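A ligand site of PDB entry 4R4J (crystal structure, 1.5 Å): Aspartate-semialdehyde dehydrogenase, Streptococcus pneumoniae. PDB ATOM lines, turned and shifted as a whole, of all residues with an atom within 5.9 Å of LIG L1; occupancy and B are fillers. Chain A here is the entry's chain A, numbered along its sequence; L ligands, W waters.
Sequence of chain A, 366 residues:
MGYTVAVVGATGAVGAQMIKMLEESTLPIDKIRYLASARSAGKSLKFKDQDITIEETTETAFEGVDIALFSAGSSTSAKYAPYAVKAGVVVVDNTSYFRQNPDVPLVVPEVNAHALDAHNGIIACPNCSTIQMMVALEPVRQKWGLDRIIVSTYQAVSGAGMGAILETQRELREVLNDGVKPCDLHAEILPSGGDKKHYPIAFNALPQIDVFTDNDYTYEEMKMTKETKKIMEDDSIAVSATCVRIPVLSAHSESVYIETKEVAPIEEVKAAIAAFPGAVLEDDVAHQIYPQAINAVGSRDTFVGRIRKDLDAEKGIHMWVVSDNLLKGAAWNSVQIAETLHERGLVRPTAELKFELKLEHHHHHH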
ATOM      1  N   GLY A  73     -16.527 -28.230 -22.022  1.00  0.00           N
ATOM      2  CA  GLY A  73     -15.251 -27.565 -21.889  1.00  0.00           C
ATOM      3  C   GLY A  73     -15.307 -26.151 -22.436  1.00  0.00           C
ATOM      4  O   GLY A  73     -16.082 -25.872 -23.353  1.00  0.00           O
ATOM      5  N   SER A  74     -14.468 -25.289 -21.880  1.00  0.00           N
ATOM      6  CA  SER A  74     -14.438 -23.868 -22.236  1.00  0.00           C
ATOM      7  C   SER A  74     -14.238 -23.623 -23.727  1.00  0.00           C
ATOM      8  O   SER A  74     -14.907 -22.784 -24.321  1.00  0.00           O
ATOM      9  CB  SER A  74     -13.337 -23.139 -21.456  1.00  0.00           C
ATOM     10  OG  SER A  74     -13.781 -22.820 -20.145  1.00  0.00           O
ATOM     11  N   ASN A  94     -22.083 -24.255 -18.584  1.00  0.00           N
ATOM     12  CA  ASN A  94     -21.479 -24.715 -17.351  1.00  0.00           C
ATOM     13  C   ASN A  94     -19.994 -24.300 -17.197  1.00  0.00           C
ATOM     14  O   ASN A  94     -19.414 -24.422 -16.107  1.00  0.00           O
ATOM     15  CB  ASN A  94     -21.614 -26.231 -17.277  1.00  0.00           C
ATOM     16  CG  ASN A  94     -21.575 -26.758 -15.877  1.00  0.00           C
ATOM     17  OD1 ASN A  94     -22.082 -26.132 -14.940  1.00  0.00           O
ATOM     18  ND2 ASN A  94     -20.969 -27.921 -15.712  1.00  0.00           N
ATOM     19  N   THR A  95     -19.409 -23.793 -18.274  1.00  0.00           N
ATOM     20  CA  THR A  95     -17.960 -23.504 -18.306  1.00  0.00           C
ATOM     21  C   THR A  95     -17.621 -22.118 -17.781  1.00  0.00           C
ATOM     22  O   THR A  95     -18.500 -21.285 -17.569  1.00  0.00           O
ATOM     23  CB  THR A  95     -17.326 -23.684 -19.712  1.00  0.00           C
ATOM     24  OG1 THR A  95     -17.526 -22.497 -20.511  1.00  0.00           O
ATOM     25  CG2 THR A  95     -17.873 -24.910 -20.441  1.00  0.00           C
ATOM     26  N   SER A  96     -16.335 -21.864 -17.609  1.00  0.00           N
ATOM     27  CA  SER A  96     -15.875 -20.567 -17.099  1.00  0.00           C
ATOM     28  C   SER A  96     -15.816 -19.479 -18.179  1.00  0.00           C
ATOM     29  O   SER A  96     -15.628 -18.304 -17.859  1.00  0.00           O
ATOM     30  CB  SER A  96     -14.484 -20.715 -16.483  1.00  0.00           C
ATOM     31  OG  SER A  96     -13.547 -21.085 -17.469  1.00  0.00           O
ATOM     32  N   TYR A  97     -15.995 -19.868 -19.449  1.00  0.00           N
ATOM     33  CA  TYR A  97     -15.598 -19.000 -20.552  1.00  0.00           C
ATOM     34  C   TYR A  97     -16.320 -17.650 -20.596  1.00  0.00           C
ATOM     35  O   TYR A  97     -15.700 -16.631 -20.843  1.00  0.00           O
ATOM     36  CB  TYR A  97     -15.754 -19.703 -21.911  1.00  0.00           C
ATOM     37  CG  TYR A  97     -15.073 -18.923 -23.006  1.00  0.00           C
ATOM     38  CD1 TYR A  97     -13.692 -18.979 -23.161  1.00  0.00           C
ATOM     39  CD2 TYR A  97     -15.803 -18.085 -23.856  1.00  0.00           C
ATOM     40  CE1 TYR A  97     -13.052 -18.243 -24.151  1.00  0.00           C
ATOM     41  CE2 TYR A  97     -15.163 -17.349 -24.845  1.00  0.00           C
ATOM     42  CZ  TYR A  97     -13.800 -17.427 -24.984  1.00  0.00           C
ATOM     43  OH  TYR A  97     -13.174 -16.708 -25.970  1.00  0.00           O
ATOM     44  N   ARG A  99     -18.303 -16.398 -18.006  1.00  0.00           N
ATOM     45  CA  ARG A  99     -18.800 -16.018 -16.682  1.00  0.00           C
ATOM     46  C   ARG A  99     -18.596 -14.548 -16.335  1.00  0.00           C
ATOM     47  O   ARG A  99     -19.438 -13.970 -15.675  1.00  0.00           O
ATOM     48  CB  ARG A  99     -18.154 -16.853 -15.578  1.00  0.00           C
ATOM     49  CG  ARG A  99     -18.559 -18.310 -15.596  1.00  0.00           C
ATOM     50  CD  ARG A  99     -18.058 -19.060 -14.372  1.00  0.00           C
ATOM     51  NE  ARG A  99     -18.388 -20.463 -14.504  1.00  0.00           N
ATOM     52  CZ  ARG A  99     -17.589 -21.478 -14.192  1.00  0.00           C
ATOM     53  NH1 ARG A  99     -16.387 -21.286 -13.669  1.00  0.00           N
ATOM     54  NH2 ARG A  99     -18.001 -22.711 -14.429  1.00  0.00           N
ATOM     55  N   PRO A 126     -22.099 -20.764 -12.486  1.00  0.00           N
ATOM     56  CA  PRO A 126     -20.782 -20.571 -11.871  1.00  0.00           C
ATOM     57  C   PRO A 126     -20.047 -21.872 -11.596  1.00  0.00           C
ATOM     58  O   PRO A 126     -20.562 -22.969 -11.820  1.00  0.00           O
ATOM     59  CB  PRO A 126     -21.090 -19.843 -10.556  1.00  0.00           C
ATOM     60  CG  PRO A 126     -22.506 -19.404 -10.647  1.00  0.00           C
ATOM     61  CD  PRO A 126     -23.177 -20.377 -11.558  1.00  0.00           C
ATOM     62  N   ASN A 127     -18.808 -21.737 -11.154  1.00  0.00           N
ATOM     63  CA  ASN A 127     -18.033 -22.834 -10.646  1.00  0.00           C
ATOM     64  C   ASN A 127     -18.756 -23.552  -9.493  1.00  0.00           C
ATOM     65  O   ASN A 127     -19.384 -22.907  -8.655  1.00  0.00           O
ATOM     66  CB  ASN A 127     -16.679 -22.282 -10.194  1.00  0.00           C
ATOM     67  CG  ASN A 127     -15.835 -23.292  -9.493  1.00  0.00           C
ATOM     68  OD1 ASN A 127     -15.816 -23.334  -8.278  1.00  0.00           O
ATOM     69  ND2 ASN A 127     -15.140 -24.115 -10.259  1.00  0.00           N
ATOM     70  N   CYS A 128     -18.660 -24.880  -9.461  1.00  0.00           N
ATOM     71  CA  CYS A 128     -19.313 -25.698  -8.434  1.00  0.00           C
ATOM     72  C   CYS A 128     -18.990 -25.251  -7.004  1.00  0.00           C
ATOM     73  O   CYS A 128     -19.883 -25.140  -6.156  1.00  0.00           O
ATOM     74  CB  CYS A 128     -18.925 -27.181  -8.595  1.00  0.00           C
ATOM     75  SG  CYS A 128     -17.168 -27.496  -8.936  1.00  0.00           S
ATOM     76  N   SER A 129     -17.720 -24.973  -6.736  1.00  0.00           N
ATOM     77  CA  SER A 129     -17.312 -24.553  -5.391  1.00  0.00           C
ATOM     78  C   SER A 129     -17.960 -23.227  -5.009  1.00  0.00           C
ATOM     79  O   SER A 129     -18.371 -23.033  -3.864  1.00  0.00           O
ATOM     80  CB  SER A 129     -15.794 -24.422  -5.292  1.00  0.00           C
ATOM     81  OG  SER A 129     -15.158 -25.640  -5.618  1.00  0.00           O
ATOM     82  N   GLN A 155     -12.144 -30.739  -2.352  1.00  0.00           N
ATOM     83  CA  GLN A 155     -12.849 -30.971  -3.603  1.00  0.00           C
ATOM     84  C   GLN A 155     -12.696 -32.392  -4.130  1.00  0.00           C
ATOM     85  O   GLN A 155     -11.612 -32.964  -4.104  1.00  0.00           O
ATOM     86  CB  GLN A 155     -12.404 -29.933  -4.642  1.00  0.00           C
ATOM     87  CG  GLN A 155     -12.959 -28.549  -4.309  1.00  0.00           C
ATOM     88  CD  GLN A 155     -12.626 -27.431  -5.285  1.00  0.00           C
ATOM     89  OE1 GLN A 155     -12.084 -26.397  -4.896  1.00  0.00           O
ATOM     90  NE2 GLN A 155     -12.975 -27.603  -6.548  1.00  0.00           N
ATOM     91  N   ALA A 156     -13.826 -32.952  -4.567  1.00  0.00           N
ATOM     92  CA  ALA A 156     -13.920 -34.270  -5.166  1.00  0.00           C
ATOM     93  C   ALA A 156     -13.323 -34.312  -6.573  1.00  0.00           C
ATOM     94  O   ALA A 156     -13.369 -33.347  -7.304  1.00  0.00           O
ATOM     95  CB  ALA A 156     -15.379 -34.698  -5.205  1.00  0.00           C
ATOM     96  N   SER A 158     -14.360 -35.838  -9.247  1.00  0.00           N
ATOM     97  CA  SER A 158     -15.280 -35.770 -10.399  1.00  0.00           C
ATOM     98  C   SER A 158     -15.379 -34.357 -10.984  1.00  0.00           C
ATOM     99  O   SER A 158     -15.798 -34.192 -12.119  1.00  0.00           O
ATOM    100  CB  SER A 158     -16.673 -36.294 -10.042  1.00  0.00           C
ATOM    101  OG  SER A 158     -17.278 -35.469  -9.060  1.00  0.00           O
ATOM    102  N   GLY A 159     -14.958 -33.341 -10.232  1.00  0.00           N
ATOM    103  CA  GLY A 159     -14.874 -31.984 -10.750  1.00  0.00           C
ATOM    104  C   GLY A 159     -13.885 -31.847 -11.896  1.00  0.00           C
ATOM    105  O   GLY A 159     -14.018 -30.954 -12.721  1.00  0.00           O
ATOM    106  N   ALA A 160     -12.906 -32.752 -11.950  1.00  0.00           N
ATOM    107  CA  ALA A 160     -11.940 -32.797 -13.046  1.00  0.00           C
ATOM    108  C   ALA A 160     -12.323 -33.739 -14.215  1.00  0.00           C
ATOM    109  O   ALA A 160     -11.553 -33.894 -15.161  1.00  0.00           O
ATOM    110  CB  ALA A 160     -10.564 -33.170 -12.502  1.00  0.00           C
ATOM    111  N   ILE A 209      -5.946 -26.782  -7.906  1.00  0.00           N
ATOM    112  CA  ILE A 209      -7.060 -27.041  -8.811  1.00  0.00           C
ATOM    113  C   ILE A 209      -6.973 -25.986  -9.907  1.00  0.00           C
ATOM    114  O   ILE A 209      -6.813 -24.786  -9.632  1.00  0.00           O
ATOM    115  CB  ILE A 209      -8.416 -27.032  -8.069  1.00  0.00           C
ATOM    116  CG1 ILE A 209      -8.388 -28.173  -7.054  1.00  0.00           C
ATOM    117  CG2 ILE A 209      -9.582 -27.152  -9.051  1.00  0.00           C
ATOM    118  CD1 ILE A 209      -9.649 -28.403  -6.278  1.00  0.00           C
ATOM    119  N   ASP A 210      -7.060 -26.450 -11.137  1.00  0.00           N
ATOM    120  CA  ASP A 210      -6.761 -25.650 -12.327  1.00  0.00           C
ATOM    121  C   ASP A 210      -5.282 -25.234 -12.344  1.00  0.00           C
ATOM    122  O   ASP A 210      -4.470 -25.805 -11.609  1.00  0.00           O
ATOM    123  CB  ASP A 210      -7.694 -24.423 -12.411  1.00  0.00           C
ATOM    124  CG  ASP A 210      -8.116 -24.101 -13.837  1.00  0.00           C
ATOM    125  OD1 ASP A 210      -7.264 -23.704 -14.645  1.00  0.00           O
ATOM    126  OD2 ASP A 210      -9.320 -24.223 -14.140  1.00  0.00           O
ATOM    127  N   GLU A 220      -8.862 -21.681 -10.099  1.00  0.00           N
ATOM    128  CA  GLU A 220     -10.010 -22.112  -9.290  1.00  0.00           C
ATOM    129  C   GLU A 220     -10.246 -21.159  -8.129  1.00  0.00           C
ATOM    130  O   GLU A 220     -11.382 -20.761  -7.856  1.00  0.00           O
ATOM    131  CB  GLU A 220      -9.816 -23.537  -8.772  1.00  0.00           C
ATOM    132  CG  GLU A 220     -10.964 -24.097  -7.928  1.00  0.00           C
ATOM    133  CD  GLU A 220     -12.174 -24.497  -8.743  1.00  0.00           C
ATOM    134  OE1 GLU A 220     -12.156 -24.334  -9.985  1.00  0.00           O
ATOM    135  OE2 GLU A 220     -13.151 -24.969  -8.099  1.00  0.00           O
ATOM    136  N   LYS A 223     -11.502 -17.846  -9.432  1.00  0.00           N
ATOM    137  CA  LYS A 223     -12.907 -17.979  -9.824  1.00  0.00           C
ATOM    138  C   LYS A 223     -13.818 -17.797  -8.629  1.00  0.00           C
ATOM    139  O   LYS A 223     -14.833 -17.104  -8.730  1.00  0.00           O
ATOM    140  CB  LYS A 223     -13.188 -19.334 -10.447  1.00  0.00           C
ATOM    141  CG  LYS A 223     -12.761 -19.497 -11.890  1.00  0.00           C
ATOM    142  CD  LYS A 223     -12.953 -20.952 -12.284  1.00  0.00           C
ATOM    143  CE  LYS A 223     -12.149 -21.352 -13.503  1.00  0.00           C
ATOM    144  NZ  LYS A 223     -12.103 -22.840 -13.573  1.00  0.00           N
ATOM    145  N   GLU A 227     -16.250 -14.734  -9.083  1.00  0.00           N
ATOM    146  CA  GLU A 227     -17.635 -15.150  -9.266  1.00  0.00           C
ATOM    147  C   GLU A 227     -18.497 -14.716  -8.088  1.00  0.00           C
ATOM    148  O   GLU A 227     -19.632 -14.271  -8.280  1.00  0.00           O
ATOM    149  CB  GLU A 227     -17.718 -16.656  -9.530  1.00  0.00           C
ATOM    150  CG  GLU A 227     -17.090 -17.032 -10.879  1.00  0.00           C
ATOM    151  CD  GLU A 227     -16.993 -18.526 -11.100  1.00  0.00           C
ATOM    152  OE1 GLU A 227     -17.731 -19.268 -10.443  1.00  0.00           O
ATOM    153  OE2 GLU A 227     -16.178 -18.951 -11.945  1.00  0.00           O
ATOM    154  N   ARG A 245      -7.682 -30.602  -3.788  1.00  0.00           N
ATOM    155  CA  ARG A 245      -8.293 -31.851  -4.229  1.00  0.00           C
ATOM    156  C   ARG A 245      -8.001 -32.942  -3.193  1.00  0.00           C
ATOM    157  O   ARG A 245      -6.848 -33.083  -2.774  1.00  0.00           O
ATOM    158  CB  ARG A 245      -7.720 -32.285  -5.566  1.00  0.00           C
ATOM    159  CG  ARG A 245      -8.524 -33.400  -6.211  1.00  0.00           C
ATOM    160  CD  ARG A 245      -9.777 -32.866  -6.900  1.00  0.00           C
ATOM    161  NE  ARG A 245      -9.438 -32.032  -8.054  1.00  0.00           N
ATOM    162  CZ  ARG A 245     -10.315 -31.328  -8.760  1.00  0.00           C
ATOM    163  NH1 ARG A 245     -11.618 -31.381  -8.480  1.00  0.00           N
ATOM    164  NH2 ARG A 245      -9.887 -30.592  -9.780  1.00  0.00           N
ATOM    165  N   HIS A 252     -18.238 -31.764  -3.023  1.00  0.00           N
ATOM    166  CA  HIS A 252     -17.236 -30.846  -2.506  1.00  0.00           C
ATOM    167  C   HIS A 252     -17.623 -30.407  -1.111  1.00  0.00           C
ATOM    168  O   HIS A 252     -18.807 -30.157  -0.836  1.00  0.00           O
ATOM    169  CB  HIS A 252     -17.133 -29.571  -3.335  1.00  0.00           C
ATOM    170  CG  HIS A 252     -16.578 -29.757  -4.719  1.00  0.00           C
ATOM    171  ND1 HIS A 252     -15.930 -30.899  -5.133  1.00  0.00           N
ATOM    172  CD2 HIS A 252     -16.527 -28.906  -5.770  1.00  0.00           C
ATOM    173  CE1 HIS A 252     -15.531 -30.754  -6.378  1.00  0.00           C
ATOM    174  NE2 HIS A 252     -15.880 -29.551  -6.797  1.00  0.00           N
ATOM    175  N   ASN A 325     -21.058 -31.831  -6.328  1.00  0.00           N
ATOM    176  CA  ASN A 325     -20.493 -30.922  -7.304  1.00  0.00           C
ATOM    177  C   ASN A 325     -21.005 -31.149  -8.732  1.00  0.00           C
ATOM    178  O   ASN A 325     -20.838 -30.268  -9.563  1.00  0.00           O
ATOM    179  CB  ASN A 325     -18.966 -31.032  -7.312  1.00  0.00           C
ATOM    180  CG  ASN A 325     -18.497 -32.430  -7.587  1.00  0.00           C
ATOM    181  OD1 ASN A 325     -18.745 -33.332  -6.782  1.00  0.00           O
ATOM    182  ND2 ASN A 325     -17.851 -32.636  -8.727  1.00  0.00           N
HETATM  183  C1  LIG L   1     -15.158 -24.692 -14.113  1.00  0.00           C
HETATM  184  C2  LIG L   1     -13.973 -26.890 -13.940  1.00  0.00           C
HETATM  185  C3  LIG L   1     -14.194 -25.711 -14.643  1.00  0.00           C
HETATM  186  C4  LIG L   1     -12.409 -27.596 -15.637  1.00  0.00           C
HETATM  187  C5  LIG L   1     -13.519 -25.481 -15.845  1.00  0.00           C
HETATM  188  O1  LIG L   1     -12.444 -29.349 -10.469  1.00  0.00           O
HETATM  189  O2  LIG L   1     -13.869 -29.396  -8.797  1.00  0.00           O
HETATM  190  C6  LIG L   1     -13.384 -28.854  -9.805  1.00  0.00           C
HETATM  191  C7  LIG L   1     -13.998 -27.534 -10.197  1.00  0.00           C
HETATM  192  C8  LIG L   1     -13.561 -27.025 -11.554  1.00  0.00           C
HETATM  193  C9  LIG L   1     -14.631 -27.240 -12.628  1.00  0.00           C
HETATM  194  C10 LIG L   1     -13.074 -27.830 -14.442  1.00  0.00           C
HETATM  195  C11 LIG L   1     -12.633 -26.426 -16.337  1.00  0.00           C
HETATM  196  O3  LIG L   1     -16.365 -24.965 -14.181  1.00  0.00           O
HETATM  197  O4  LIG L   1     -14.750 -23.607 -13.633  1.00  0.00           O
HETATM  198  C12 LIG L   1     -13.703 -24.258 -16.687  1.00  0.00           C
HETATM  199  O5  LIG L   1     -12.796 -23.387 -16.701  1.00  0.00           O
HETATM  200  O6  LIG L   1     -14.743 -24.158 -17.386  1.00  0.00           O
HETATM  201  P1  LG2 L   2     -15.519 -34.946 -18.896  1.00  0.00           P
HETATM  202  O1  LG2 L   2     -14.076 -34.988 -19.335  1.00  0.00           O
HETATM  203  O2  LG2 L   2     -16.089 -35.986 -17.960  1.00  0.00           O
HETATM  204  O3  LG2 L   2     -16.433 -34.854 -20.205  1.00  0.00           O
HETATM  205  C1  LG2 L   2     -16.067 -33.984 -21.260  1.00  0.00           C
HETATM  206  C2  LG2 L   2     -17.249 -33.861 -22.201  1.00  0.00           C
HETATM  207  O4  LG2 L   2     -16.907 -32.819 -23.139  1.00  0.00           O
HETATM  208  C3  LG2 L   2     -17.530 -35.133 -23.004  1.00  0.00           C
HETATM  209  O5  LG2 L   2     -18.930 -35.272 -23.275  1.00  0.00           O
HETATM  210  C4  LG2 L   2     -16.773 -34.843 -24.291  1.00  0.00           C
HETATM  211  O6  LG2 L   2     -17.202 -35.604 -25.434  1.00  0.00           O
HETATM  212  C5  LG2 L   2     -17.043 -33.347 -24.438  1.00  0.00           C
HETATM  213  N1  LG2 L   2     -16.102 -32.735 -25.384  1.00  0.00           N
HETATM  214  C6  LG2 L   2     -14.753 -32.700 -25.308  1.00  0.00           C
HETATM  215  N2  LG2 L   2     -14.239 -32.093 -26.399  1.00  0.00           N
HETATM  216  C7  LG2 L   2     -15.268 -31.743 -27.184  1.00  0.00           C
HETATM  217  C8  LG2 L   2     -15.443 -31.068 -28.495  1.00  0.00           C
HETATM  218  N3  LG2 L   2     -14.375 -30.631 -29.211  1.00  0.00           N
HETATM  219  N4  LG2 L   2     -16.710 -30.910 -28.948  1.00  0.00           N
HETATM  220  C9  LG2 L   2     -17.791 -31.331 -28.261  1.00  0.00           C
HETATM  221  N5  LG2 L   2     -17.705 -31.958 -27.076  1.00  0.00           N
HETATM  222  C10 LG2 L   2     -16.492 -32.177 -26.513  1.00  0.00           C
HETATM  223  O7  LG2 L   2     -15.694 -33.488 -18.235  1.00  0.00           O
HETATM  224  P2  LG2 L   2     -16.889 -33.001 -17.252  1.00  0.00           P
HETATM  225  O8  LG2 L   2     -16.457 -33.219 -15.830  1.00  0.00           O
HETATM  226  O9  LG2 L   2     -18.212 -33.526 -17.730  1.00  0.00           O
HETATM  227  O10 LG2 L   2     -16.791 -31.437 -17.510  1.00  0.00           O
HETATM  228  C11 LG2 L   2     -16.760 -30.876 -18.815  1.00  0.00           C
HETATM  229  C12 LG2 L   2     -16.738 -29.374 -18.612  1.00  0.00           C
HETATM  230  O11 LG2 L   2     -17.854 -28.995 -17.805  1.00  0.00           O
HETATM  231  C13 LG2 L   2     -15.511 -28.889 -17.856  1.00  0.00           C
HETATM  232  O12 LG2 L   2     -14.377 -28.705 -18.709  1.00  0.00           O
HETATM  233  C14 LG2 L   2     -16.042 -27.591 -17.266  1.00  0.00           C
HETATM  234  O13 LG2 L   2     -15.875 -26.522 -18.184  1.00  0.00           O
HETATM  235  C15 LG2 L   2     -17.522 -27.860 -17.022  1.00  0.00           C
HETATM  236  N6  LG2 L   2     -17.733 -28.134 -15.597  1.00  0.00           N
HETATM  237  C16 LG2 L   2     -18.223 -27.158 -14.834  1.00  0.00           C
HETATM  238  C17 LG2 L   2     -18.440 -27.366 -13.477  1.00  0.00           C
HETATM  239  C18 LG2 L   2     -18.951 -26.279 -12.617  1.00  0.00           C
HETATM  240  O14 LG2 L   2     -18.311 -26.092 -11.595  1.00  0.00           O
HETATM  241  N7  LG2 L   2     -20.026 -25.562 -12.960  1.00  0.00           N
HETATM  242  C19 LG2 L   2     -18.116 -28.577 -12.898  1.00  0.00           C
HETATM  243  C20 LG2 L   2     -17.599 -29.573 -13.703  1.00  0.00           C
HETATM  244  C21 LG2 L   2     -17.398 -29.327 -15.055  1.00  0.00           C
HETATM  245  P3  LG2 L   2     -16.481 -36.976 -25.906  1.00  0.00           P
HETATM  246  O15 LG2 L   2     -16.993 -38.026 -24.959  1.00  0.00           O
HETATM  247  O16 LG2 L   2     -16.930 -37.156 -27.341  1.00  0.00           O
HETATM  248  O17 LG2 L   2     -15.006 -36.678 -25.755  1.00  0.00           O
HETATM  249  O   HOH W   1     -12.956 -26.263 -19.725  1.00  0.00           O
HETATM  250  O   HOH W   2     -10.688 -28.996 -12.414  1.00  0.00           O
HETATM  251  O   HOH W   3     -10.737 -26.237 -12.824  1.00  0.00           O
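The side-chain sulfur (SG) of Cys 128 is in hydrogen-bond range of an oxygen (O14) of LG2 L2, 3.2 Å away. The side-chain amide oxygen of Asn 94 lies within hydrogen-bond range of a nitrogen (N7) of LG2 L2, 2.9 Å away. The guanidinium group (NH2) of Arg 99 lies within salt-bridge range of an oxygen (O3) of LIG L1, at 2.8 Å. An oxygen (O1) of LIG L1 is in salt-bridge range of the guanidinium group (NH2) of Arg 245 (2.9 Å). A nitrogen (N7) of LG2 L2 lies close to the backbone carbonyl oxygen (O) of Asn 94 (3.4 Å). The backbone carbonyl oxygen of Pro 126 is in hydrogen-bond range of a nitrogen (N7) of LG2 L2 (2.9 Å). The backbone NH (N) of Cys 128 sits at hydrogen-bond distance from an oxygen (O14) of LG2 L2, 2.5 Å away. N of Ser 96 lies within hydrogen-bond range of O6 of LIG L1 (2.8 Å). An oxygen (O4) of LIG L1 lies within hydrogen-bond range of the side-chain amide nitrogen (ND2) of Asn 127 (3.4 Å). The side-chain hydroxyl (OG) of Ser 74 sits at hydrogen-bond distance from an oxygen (O6) of LIG L1 (3.2 Å). A ring nitrogen (NE2) of His 252 lies within hydrogen-bond range of an oxygen (O2) of LIG L1, 2.8 Å away. An oxygen (O4) of LIG L1 lies within salt-bridge range of the side-chain amino group (NZ) of Lys 223 (2.8 Å). The side-chain hydroxyl (OG) of Ser 96 is in hydrogen-bond range of an oxygen (O5) of LIG L1 (2.5 Å). The side-chain amide nitrogen (NE2) of Gln 155 sits at hydrogen-bond distance from an oxygen (O2) of LIG L1 (3.0 Å).
An oxygen (O6) of LIG L1 lies within hydrogen-bond range of an oxygen (O13) of LG2 L2 (2.7 Å).
NH2 of Arg 99 lies within hydrogen-bond range of O of Asn 94 (2.8 Å). The guanidinium group (NH1) of Arg 245 lies within hydrogen-bond range of the backbone carbonyl oxygen (O) of Ala 156, 2.9 Å away. The side-chain carboxylate (OE1) of Glu 220 sits at hydrogen-bond distance from the side-chain amide nitrogen (ND2) of Asn 127, 3.0 Å away. A ring nitrogen (ND1) of His 252 lies within hydrogen-bond range of the backbone NH (N) of Ala 156 (3.0 Å). The side-chain amide nitrogen (ND2) of Asn 325 sits close to the backbone NH (N) of Gly 159, 3.3 Å away. OD1 of Asn 127 sits at hydrogen-bond distance from N of Ser 129, 2.9 Å away. The side-chain amino group of Lys 223 is in salt-bridge range of the side-chain carboxylate of Glu 220, 3.9 Å away. OE2 of Glu 220 lies within hydrogen-bond range of OG of Ser 129.
O of Gly 159 sits close to O1 of LIG L1 (3.2 Å). O of Asn 94 touches O3 of LIG L1 (3.6 Å). Thr 95 touches LIG L1 (CA to O6, 3.4 Å). Cys 128 touches LIG L1 (SG to C7, 3.4 Å). N of Ala 160 touches O1 of LIG L1, at 3.7 Å. CG2 of Ile 209 touches O1 of LIG L1, 3.9 Å away. OE1 of Glu 220 touches C8 of LIG L1 (3.4 Å). Hydrophobic or aromatic side chains that line LIG L1: Ile 209 and His 252. 15 residues have an atom within 4 Å of LIG L1: Ser 74, Asn 94, Thr 95, Ser 96, Arg 99, Asn 127, Cys 128, Gln 155, Gly 159, Ala 160, Ile 209, Glu 220, Lys 223, Arg 245 and His 252. The nearest printed residue that does not touch LIG L1 is Ala 156 (4.3 Å).
Water W2 bridges an oxygen (O1) of LIG L1 and the guanidinium group of Arg 245. Water W1 lies within hydrogen-bond range of the backbone NH (N) of Ser 74 (2.8 Å) and an oxygen (O12) of LG2 L2 (3.0 Å).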
